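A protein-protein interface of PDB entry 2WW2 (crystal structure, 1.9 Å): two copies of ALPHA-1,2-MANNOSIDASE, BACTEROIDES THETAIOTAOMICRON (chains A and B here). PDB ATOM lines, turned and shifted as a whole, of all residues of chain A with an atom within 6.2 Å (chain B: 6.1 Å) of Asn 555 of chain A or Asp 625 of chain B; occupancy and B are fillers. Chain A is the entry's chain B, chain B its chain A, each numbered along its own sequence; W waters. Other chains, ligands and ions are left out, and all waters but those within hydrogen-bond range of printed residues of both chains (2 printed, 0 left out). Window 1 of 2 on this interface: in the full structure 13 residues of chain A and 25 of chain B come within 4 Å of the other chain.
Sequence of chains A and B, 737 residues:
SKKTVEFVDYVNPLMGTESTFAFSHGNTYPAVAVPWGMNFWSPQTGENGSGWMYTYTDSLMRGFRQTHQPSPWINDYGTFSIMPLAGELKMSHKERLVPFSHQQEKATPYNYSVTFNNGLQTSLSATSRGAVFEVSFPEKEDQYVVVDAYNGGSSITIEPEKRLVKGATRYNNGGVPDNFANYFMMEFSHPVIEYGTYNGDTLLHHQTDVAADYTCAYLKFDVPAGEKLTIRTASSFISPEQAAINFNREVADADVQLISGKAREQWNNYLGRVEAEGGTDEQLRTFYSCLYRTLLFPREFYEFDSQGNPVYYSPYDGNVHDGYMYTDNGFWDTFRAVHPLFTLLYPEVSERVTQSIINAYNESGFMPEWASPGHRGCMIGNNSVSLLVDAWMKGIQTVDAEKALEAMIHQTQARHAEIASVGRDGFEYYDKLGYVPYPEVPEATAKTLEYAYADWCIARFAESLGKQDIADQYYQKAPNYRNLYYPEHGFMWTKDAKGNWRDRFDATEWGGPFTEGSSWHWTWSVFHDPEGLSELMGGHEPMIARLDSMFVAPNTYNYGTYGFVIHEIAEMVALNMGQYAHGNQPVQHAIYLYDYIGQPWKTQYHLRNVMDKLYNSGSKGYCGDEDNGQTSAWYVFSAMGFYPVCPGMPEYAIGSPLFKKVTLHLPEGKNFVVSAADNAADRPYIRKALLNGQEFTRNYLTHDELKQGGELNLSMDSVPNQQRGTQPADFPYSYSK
Water W2 lies within hydrogen-bond range of OD1 of Asn 555 of chain A and SG of Cys 623 of chain B. Water W1 lies within hydrogen-bond range of OH of Tyr 557 of chain A (2.8 Å), N of Asp 625 of chain B (3.0 Å) and O of Leu 575 of chain B (3.3 Å).
OD1 of Asn 576 of chain B sits at hydrogen-bond distance from OH of Tyr 557 of chain A, at 2.9 Å. O of Cys 623 of chain B lies within hydrogen-bond range of ND2 of Asn 555 of chain A, 2.8 Å away. ND2 of Asn 555 of chain A sits at hydrogen-bond distance from OD1 of Asp 625 of chain B (3.1 Å).
No position is printed for both chains.
The backbone carbonyl oxygen (O) of Met 572 of chain B sits close to the side-chain amide nitrogen (ND2) of Asn 576 of chain B (3.5 Å). N of Tyr 557 of chain A sits at hydrogen-bond distance from OD1 of Asn 555 of chain A (2.9 Å).
Asn 576 of chain B touches Asn 555 of chain A (ND2 to O, 3.9 Å). CE of Met 572 of chain B touches CB of Thr 556 of chain A (3.8 Å). Tyr 557 of chain A touches Leu 575 of chain B (OH to CB, 3.4 Å). Tyr 557 of chain A touches Cys 623 of chain B. Tyr 557 of chain A touches Asp 625 of chain B. Tyr 559 of chain A touches Met 572 of chain B.
Hydrophobic or aromatic side chains of chain B within 4 Å of the printed part of chain A: Met 572 and Leu 575. Printed residues of chain A that touch a printed residue of chain B: Asn 555, Thr 556, Tyr 557 and Tyr 559. Among the printed residues, 9 pairs touch across the chains.
Asn 555 of chain A touches three residues of chain B. Of the printed residues of chain B, Thr 556 of chain A touches Met 572. Of the printed residues of chain B, Tyr 559 of chain A touches Met 572 (3.5 Å). Printed residues of chain A within 4 Å of Asn 576 of chain B: Asn 555 (3.9 Å) and Tyr 557 (2.9 Å). Of the printed residues of chain A, Cys 623 of chain B touches Asn 555 and Tyr 557. Of chain A, only Asn 555 (3.1 Å) and Tyr 557 (3.7 Å) come within 4 Å of Asp 625 of chain B. The nearest residue of chain B that does not touch Asn 555 of chain A is Met 572 of chain B (4.1 Å). The nearest printed residue of chain A that does not touch Asp 625 of chain B is Pro 554 of chain A (7.1 Å). The nearest printed residue of chain B that does not touch Tyr 557 of chain A is Met 572 of chain B (4.4 Å).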
ATOM      1  N   ALA A 553      -7.797   2.807 -30.735  1.00  0.00           N
ATOM      2  CA  ALA A 553      -8.746   3.869 -31.059  1.00  0.00           C
ATOM      3  C   ALA A 553      -9.686   4.034 -29.859  1.00  0.00           C
ATOM      4  O   ALA A 553      -9.882   3.093 -29.094  1.00  0.00           O
ATOM      5  CB  ALA A 553      -9.527   3.532 -32.336  1.00  0.00           C
ATOM      6  N   PRO A 554     -10.253   5.231 -29.680  1.00  0.00           N
ATOM      7  CA  PRO A 554     -11.006   5.499 -28.457  1.00  0.00           C
ATOM      8  C   PRO A 554     -12.332   4.760 -28.410  1.00  0.00           C
ATOM      9  O   PRO A 554     -12.900   4.428 -29.451  1.00  0.00           O
ATOM     10  CB  PRO A 554     -11.278   7.001 -28.538  1.00  0.00           C
ATOM     11  CG  PRO A 554     -11.306   7.285 -30.023  1.00  0.00           C
ATOM     12  CD  PRO A 554     -10.258   6.380 -30.607  1.00  0.00           C
ATOM     13  N   ASN A 555     -12.812   4.519 -27.195  1.00  0.00           N
ATOM     14  CA  ASN A 555     -14.098   3.876 -26.979  1.00  0.00           C
ATOM     15  C   ASN A 555     -15.241   4.872 -27.133  1.00  0.00           C
ATOM     16  O   ASN A 555     -15.294   5.886 -26.424  1.00  0.00           O
ATOM     17  CB  ASN A 555     -14.132   3.259 -25.584  1.00  0.00           C
ATOM     18  CG  ASN A 555     -15.338   2.369 -25.366  1.00  0.00           C
ATOM     19  OD1 ASN A 555     -16.249   2.309 -26.201  1.00  0.00           O
ATOM     20  ND2 ASN A 555     -15.355   1.675 -24.234  1.00  0.00           N
ATOM     21  N   THR A 556     -16.156   4.587 -28.053  1.00  0.00           N
ATOM     22  CA  THR A 556     -17.288   5.485 -28.295  1.00  0.00           C
ATOM     23  C   THR A 556     -18.631   4.918 -27.827  1.00  0.00           C
ATOM     24  O   THR A 556     -19.687   5.516 -28.091  1.00  0.00           O
ATOM     25  CB  THR A 556     -17.402   5.880 -29.797  1.00  0.00           C
ATOM     26  OG1 THR A 556     -17.552   4.704 -30.604  1.00  0.00           O
ATOM     27  CG2 THR A 556     -16.164   6.658 -30.246  1.00  0.00           C
ATOM     28  N   TYR A 557     -18.583   3.771 -27.149  1.00  0.00           N
ATOM     29  CA  TYR A 557     -19.777   3.134 -26.589  1.00  0.00           C
ATOM     30  C   TYR A 557     -20.871   2.997 -27.648  1.00  0.00           C
ATOM     31  O   TYR A 557     -20.620   2.438 -28.709  1.00  0.00           O
ATOM     32  CB  TYR A 557     -20.243   3.889 -25.332  1.00  0.00           C
ATOM     33  CG  TYR A 557     -19.101   4.054 -24.353  1.00  0.00           C
ATOM     34  CD1 TYR A 557     -18.877   3.124 -23.352  1.00  0.00           C
ATOM     35  CD2 TYR A 557     -18.199   5.115 -24.480  1.00  0.00           C
ATOM     36  CE1 TYR A 557     -17.816   3.259 -22.474  1.00  0.00           C
ATOM     37  CE2 TYR A 557     -17.131   5.258 -23.609  1.00  0.00           C
ATOM     38  CZ  TYR A 557     -16.939   4.326 -22.612  1.00  0.00           C
ATOM     39  OH  TYR A 557     -15.873   4.466 -21.742  1.00  0.00           O
ATOM     40  N   ASN A 558     -22.069   3.518 -27.381  1.00  0.00           N
ATOM     41  CA  ASN A 558     -23.136   3.527 -28.396  1.00  0.00           C
ATOM     42  C   ASN A 558     -23.329   4.876 -29.106  1.00  0.00           C
ATOM     43  O   ASN A 558     -24.303   5.067 -29.834  1.00  0.00           O
ATOM     44  CB  ASN A 558     -24.476   3.107 -27.790  1.00  0.00           C
ATOM     45  CG  ASN A 558     -24.488   1.656 -27.330  1.00  0.00           C
ATOM     46  OD1 ASN A 558     -25.065   1.328 -26.292  1.00  0.00           O
ATOM     47  ND2 ASN A 558     -23.864   0.785 -28.102  1.00  0.00           N
ATOM     48  N   TYR A 559     -22.407   5.806 -28.893  1.00  0.00           N
ATOM     49  CA  TYR A 559     -22.554   7.160 -29.423  1.00  0.00           C
ATOM     50  C   TYR A 559     -22.281   7.248 -30.924  1.00  0.00           C
ATOM     51  O   TYR A 559     -22.550   8.274 -31.549  1.00  0.00           O
ATOM     52  CB  TYR A 559     -21.695   8.147 -28.619  1.00  0.00           C
ATOM     53  CG  TYR A 559     -22.043   8.140 -27.145  1.00  0.00           C
ATOM     54  CD1 TYR A 559     -23.245   8.685 -26.688  1.00  0.00           C
ATOM     55  CD2 TYR A 559     -21.188   7.567 -26.211  1.00  0.00           C
ATOM     56  CE1 TYR A 559     -23.575   8.664 -25.331  1.00  0.00           C
ATOM     57  CE2 TYR A 559     -21.505   7.543 -24.864  1.00  0.00           C
ATOM     58  CZ  TYR A 559     -22.699   8.090 -24.427  1.00  0.00           C
ATOM     59  OH  TYR A 559     -23.003   8.050 -23.080  1.00  0.00           O
ATOM     60  N   ALA A 570     -13.640  11.730 -30.811  1.00  0.00           N
ATOM     61  CA  ALA A 570     -13.242  10.889 -29.694  1.00  0.00           C
ATOM     62  C   ALA A 570     -11.739  10.632 -29.709  1.00  0.00           C
ATOM     63  O   ALA A 570     -11.135  10.397 -28.661  1.00  0.00           O
ATOM     64  CB  ALA A 570     -14.001   9.579 -29.724  1.00  0.00           C
ATOM     65  N   SER B  19     -14.584  -6.496 -27.147  1.00  0.00           N
ATOM     66  CA  SER B  19     -14.867  -5.666 -25.967  1.00  0.00           C
ATOM     67  C   SER B  19     -14.018  -5.954 -24.755  1.00  0.00           C
ATOM     68  O   SER B  19     -14.221  -5.338 -23.702  1.00  0.00           O
ATOM     69  CB  SER B  19     -16.313  -5.885 -25.520  1.00  0.00           C
ATOM     70  OG  SER B  19     -17.166  -5.055 -26.238  1.00  0.00           O
ATOM     71  N   PHE B  21     -10.499  -6.540 -22.463  1.00  0.00           N
ATOM     72  CA  PHE B  21      -9.121  -6.128 -22.245  1.00  0.00           C
ATOM     73  C   PHE B  21      -8.202  -7.360 -22.300  1.00  0.00           C
ATOM     74  O   PHE B  21      -8.484  -8.397 -21.690  1.00  0.00           O
ATOM     75  CB  PHE B  21      -9.035  -5.419 -20.894  1.00  0.00           C
ATOM     76  CG  PHE B  21      -7.675  -4.919 -20.552  1.00  0.00           C
ATOM     77  CD1 PHE B  21      -6.967  -4.127 -21.437  1.00  0.00           C
ATOM     78  CD2 PHE B  21      -7.112  -5.215 -19.316  1.00  0.00           C
ATOM     79  CE1 PHE B  21      -5.699  -3.655 -21.107  1.00  0.00           C
ATOM     80  CE2 PHE B  21      -5.853  -4.744 -18.980  1.00  0.00           C
ATOM     81  CZ  PHE B  21      -5.147  -3.963 -19.872  1.00  0.00           C
ATOM     82  N   MET B 572     -19.338  10.582 -22.645  1.00  0.00           N
ATOM     83  CA  MET B 572     -18.168   9.747 -22.910  1.00  0.00           C
ATOM     84  C   MET B 572     -17.052  10.015 -21.902  1.00  0.00           C
ATOM     85  O   MET B 572     -16.404   9.085 -21.413  1.00  0.00           O
ATOM     86  CB  MET B 572     -17.614  10.033 -24.304  1.00  0.00           C
ATOM     87  CG  MET B 572     -18.355   9.411 -25.460  1.00  0.00           C
ATOM     88  SD  MET B 572     -17.237   9.411 -26.880  1.00  0.00           S
ATOM     89  CE  MET B 572     -18.342   9.182 -28.258  1.00  0.00           C
ATOM     90  N   LEU B 575     -17.142   8.318 -18.493  1.00  0.00           N
ATOM     91  CA  LEU B 575     -16.945   6.885 -18.668  1.00  0.00           C
ATOM     92  C   LEU B 575     -15.480   6.563 -18.955  1.00  0.00           C
ATOM     93  O   LEU B 575     -14.922   5.614 -18.405  1.00  0.00           O
ATOM     94  CB  LEU B 575     -17.851   6.359 -19.790  1.00  0.00           C
ATOM     95  CG  LEU B 575     -19.360   6.403 -19.526  1.00  0.00           C
ATOM     96  CD1 LEU B 575     -20.157   6.330 -20.827  1.00  0.00           C
ATOM     97  CD2 LEU B 575     -19.777   5.294 -18.556  1.00  0.00           C
ATOM     98  N   ASN B 576     -14.863   7.372 -19.814  1.00  0.00           N
ATOM     99  CA  ASN B 576     -13.453   7.214 -20.159  1.00  0.00           C
ATOM    100  C   ASN B 576     -12.507   7.517 -18.996  1.00  0.00           C
ATOM    101  O   ASN B 576     -11.454   6.895 -18.872  1.00  0.00           O
ATOM    102  CB  ASN B 576     -13.105   8.051 -21.393  1.00  0.00           C
ATOM    103  CG  ASN B 576     -13.668   7.453 -22.671  1.00  0.00           C
ATOM    104  OD1 ASN B 576     -13.884   6.241 -22.762  1.00  0.00           O
ATOM    105  ND2 ASN B 576     -13.908   8.298 -23.666  1.00  0.00           N
ATOM    106  N   MET B 577     -12.893   8.456 -18.135  1.00  0.00           N
ATOM    107  CA  MET B 577     -12.122   8.731 -16.922  1.00  0.00           C
ATOM    108  C   MET B 577     -12.418   7.672 -15.864  1.00  0.00           C
ATOM    109  O   MET B 577     -11.598   7.417 -14.979  1.00  0.00           O
ATOM    110  CB  MET B 577     -12.415  10.142 -16.387  1.00  0.00           C
ATOM    111  N   HIS B 582     -18.221   0.325 -14.407  1.00  0.00           N
ATOM    112  CA  HIS B 582     -19.208  -0.727 -14.614  1.00  0.00           C
ATOM    113  C   HIS B 582     -18.507  -2.057 -14.925  1.00  0.00           C
ATOM    114  O   HIS B 582     -17.692  -2.151 -15.835  1.00  0.00           O
ATOM    115  CB  HIS B 582     -20.197  -0.366 -15.725  1.00  0.00           C
ATOM    116  CG  HIS B 582     -21.283  -1.385 -15.897  1.00  0.00           C
ATOM    117  ND1 HIS B 582     -22.204  -1.657 -14.905  1.00  0.00           N
ATOM    118  CD2 HIS B 582     -21.580  -2.219 -16.927  1.00  0.00           C
ATOM    119  CE1 HIS B 582     -23.033  -2.598 -15.321  1.00  0.00           C
ATOM    120  NE2 HIS B 582     -22.677  -2.956 -16.547  1.00  0.00           N
ATOM    121  N   TYR B 622     -19.938  -5.301 -24.880  1.00  0.00           N
ATOM    122  CA  TYR B 622     -19.700  -5.036 -23.447  1.00  0.00           C
ATOM    123  C   TYR B 622     -18.850  -3.770 -23.372  1.00  0.00           C
ATOM    124  O   TYR B 622     -17.613  -3.840 -23.251  1.00  0.00           O
ATOM    125  CB  TYR B 622     -18.983  -6.219 -22.780  1.00  0.00           C
ATOM    126  CG  TYR B 622     -19.872  -7.441 -22.594  1.00  0.00           C
ATOM    127  CD1 TYR B 622     -20.767  -7.508 -21.531  1.00  0.00           C
ATOM    128  CD2 TYR B 622     -19.810  -8.527 -23.475  1.00  0.00           C
ATOM    129  CE1 TYR B 622     -21.594  -8.620 -21.334  1.00  0.00           C
ATOM    130  CE2 TYR B 622     -20.637  -9.649 -23.297  1.00  0.00           C
ATOM    131  CZ  TYR B 622     -21.530  -9.678 -22.218  1.00  0.00           C
ATOM    132  OH  TYR B 622     -22.346 -10.766 -22.014  1.00  0.00           O
ATOM    133  N   CYS B 623     -19.513  -2.612 -23.509  1.00  0.00           N
ATOM    134  CA  CYS B 623     -18.828  -1.331 -23.765  1.00  0.00           C
ATOM    135  C   CYS B 623     -17.953  -0.820 -22.632  1.00  0.00           C
ATOM    136  O   CYS B 623     -16.917  -0.196 -22.894  1.00  0.00           O
ATOM    137  CB  CYS B 623     -19.826  -0.225 -24.155  1.00  0.00           C
ATOM    138  SG  CYS B 623     -20.943  -0.696 -25.490  1.00  0.00           S
ATOM    139  N   GLY B 624     -18.368  -1.054 -21.391  1.00  0.00           N
ATOM    140  CA  GLY B 624     -17.585  -0.608 -20.235  1.00  0.00           C
ATOM    141  C   GLY B 624     -16.112  -1.009 -20.346  1.00  0.00           C
ATOM    142  O   GLY B 624     -15.795  -2.184 -20.589  1.00  0.00           O
ATOM    143  N   ASP B 625     -15.210  -0.037 -20.167  1.00  0.00           N
ATOM    144  CA  ASP B 625     -13.769  -0.309 -20.177  1.00  0.00           C
ATOM    145  C   ASP B 625     -13.422  -1.413 -19.172  1.00  0.00           C
ATOM    146  O   ASP B 625     -12.469  -2.169 -19.356  1.00  0.00           O
ATOM    147  CB  ASP B 625     -12.989   0.950 -19.794  1.00  0.00           C
ATOM    148  CG  ASP B 625     -12.901   1.947 -20.933  1.00  0.00           C
ATOM    149  OD1 ASP B 625     -13.123   1.560 -22.116  1.00  0.00           O
ATOM    150  OD2 ASP B 625     -12.604   3.123 -20.634  1.00  0.00           O
ATOM    151  N   GLU B 626     -14.213  -1.501 -18.118  1.00  0.00           N
ATOM    152  CA  GLU B 626     -13.956  -2.476 -17.077  1.00  0.00           C
ATOM    153  C   GLU B 626     -14.815  -3.710 -17.217  1.00  0.00           C
ATOM    154  O   GLU B 626     -14.794  -4.585 -16.361  1.00  0.00           O
ATOM    155  CB  GLU B 626     -14.318  -1.857 -15.755  1.00  0.00           C
ATOM    156  CG  GLU B 626     -13.526  -2.347 -14.650  1.00  0.00           C
ATOM    157  CD  GLU B 626     -12.507  -1.338 -14.300  1.00  0.00           C
ATOM    158  OE1 GLU B 626     -12.017  -0.686 -15.249  1.00  0.00           O
ATOM    159  OE2 GLU B 626     -12.231  -1.182 -13.093  1.00  0.00           O
ATOM    160  N   ASP B 627     -15.606  -3.768 -18.276  1.00  0.00           N
ATOM    161  CA  ASP B 627     -16.522  -4.889 -18.465  1.00  0.00           C
ATOM    162  C   ASP B 627     -15.980  -5.807 -19.540  1.00  0.00           C
ATOM    163  O   ASP B 627     -15.928  -5.449 -20.726  1.00  0.00           O
ATOM    164  CB  ASP B 627     -17.912  -4.395 -18.848  1.00  0.00           C
ATOM    165  CG  ASP B 627     -18.963  -5.511 -18.833  1.00  0.00           C
ATOM    166  OD1 ASP B 627     -18.600  -6.711 -18.675  1.00  0.00           O
ATOM    167  OD2 ASP B 627     -20.158  -5.178 -18.990  1.00  0.00           O
ATOM    168  N   ASN B 628     -15.548  -6.985 -19.108  1.00  0.00           N
ATOM    169  CA  ASN B 628     -14.979  -7.964 -20.014  1.00  0.00           C
ATOM    170  C   ASN B 628     -15.907  -9.165 -20.192  1.00  0.00           C
ATOM    171  O   ASN B 628     -15.454 -10.279 -20.454  1.00  0.00           O
ATOM    172  CB  ASN B 628     -13.615  -8.393 -19.483  1.00  0.00           C
ATOM    173  CG  ASN B 628     -12.681  -7.203 -19.321  1.00  0.00           C
ATOM    174  OD1 ASN B 628     -12.253  -6.853 -18.196  1.00  0.00           O
ATOM    175  ND2 ASN B 628     -12.420  -6.525 -20.432  1.00  0.00           N
HETATM  176  O   HOH W   1     -16.043   2.715 -19.501  1.00  0.00           O
HETATM  177  O   HOH W   2     -17.474  -0.134 -26.740  1.00  0.00           O
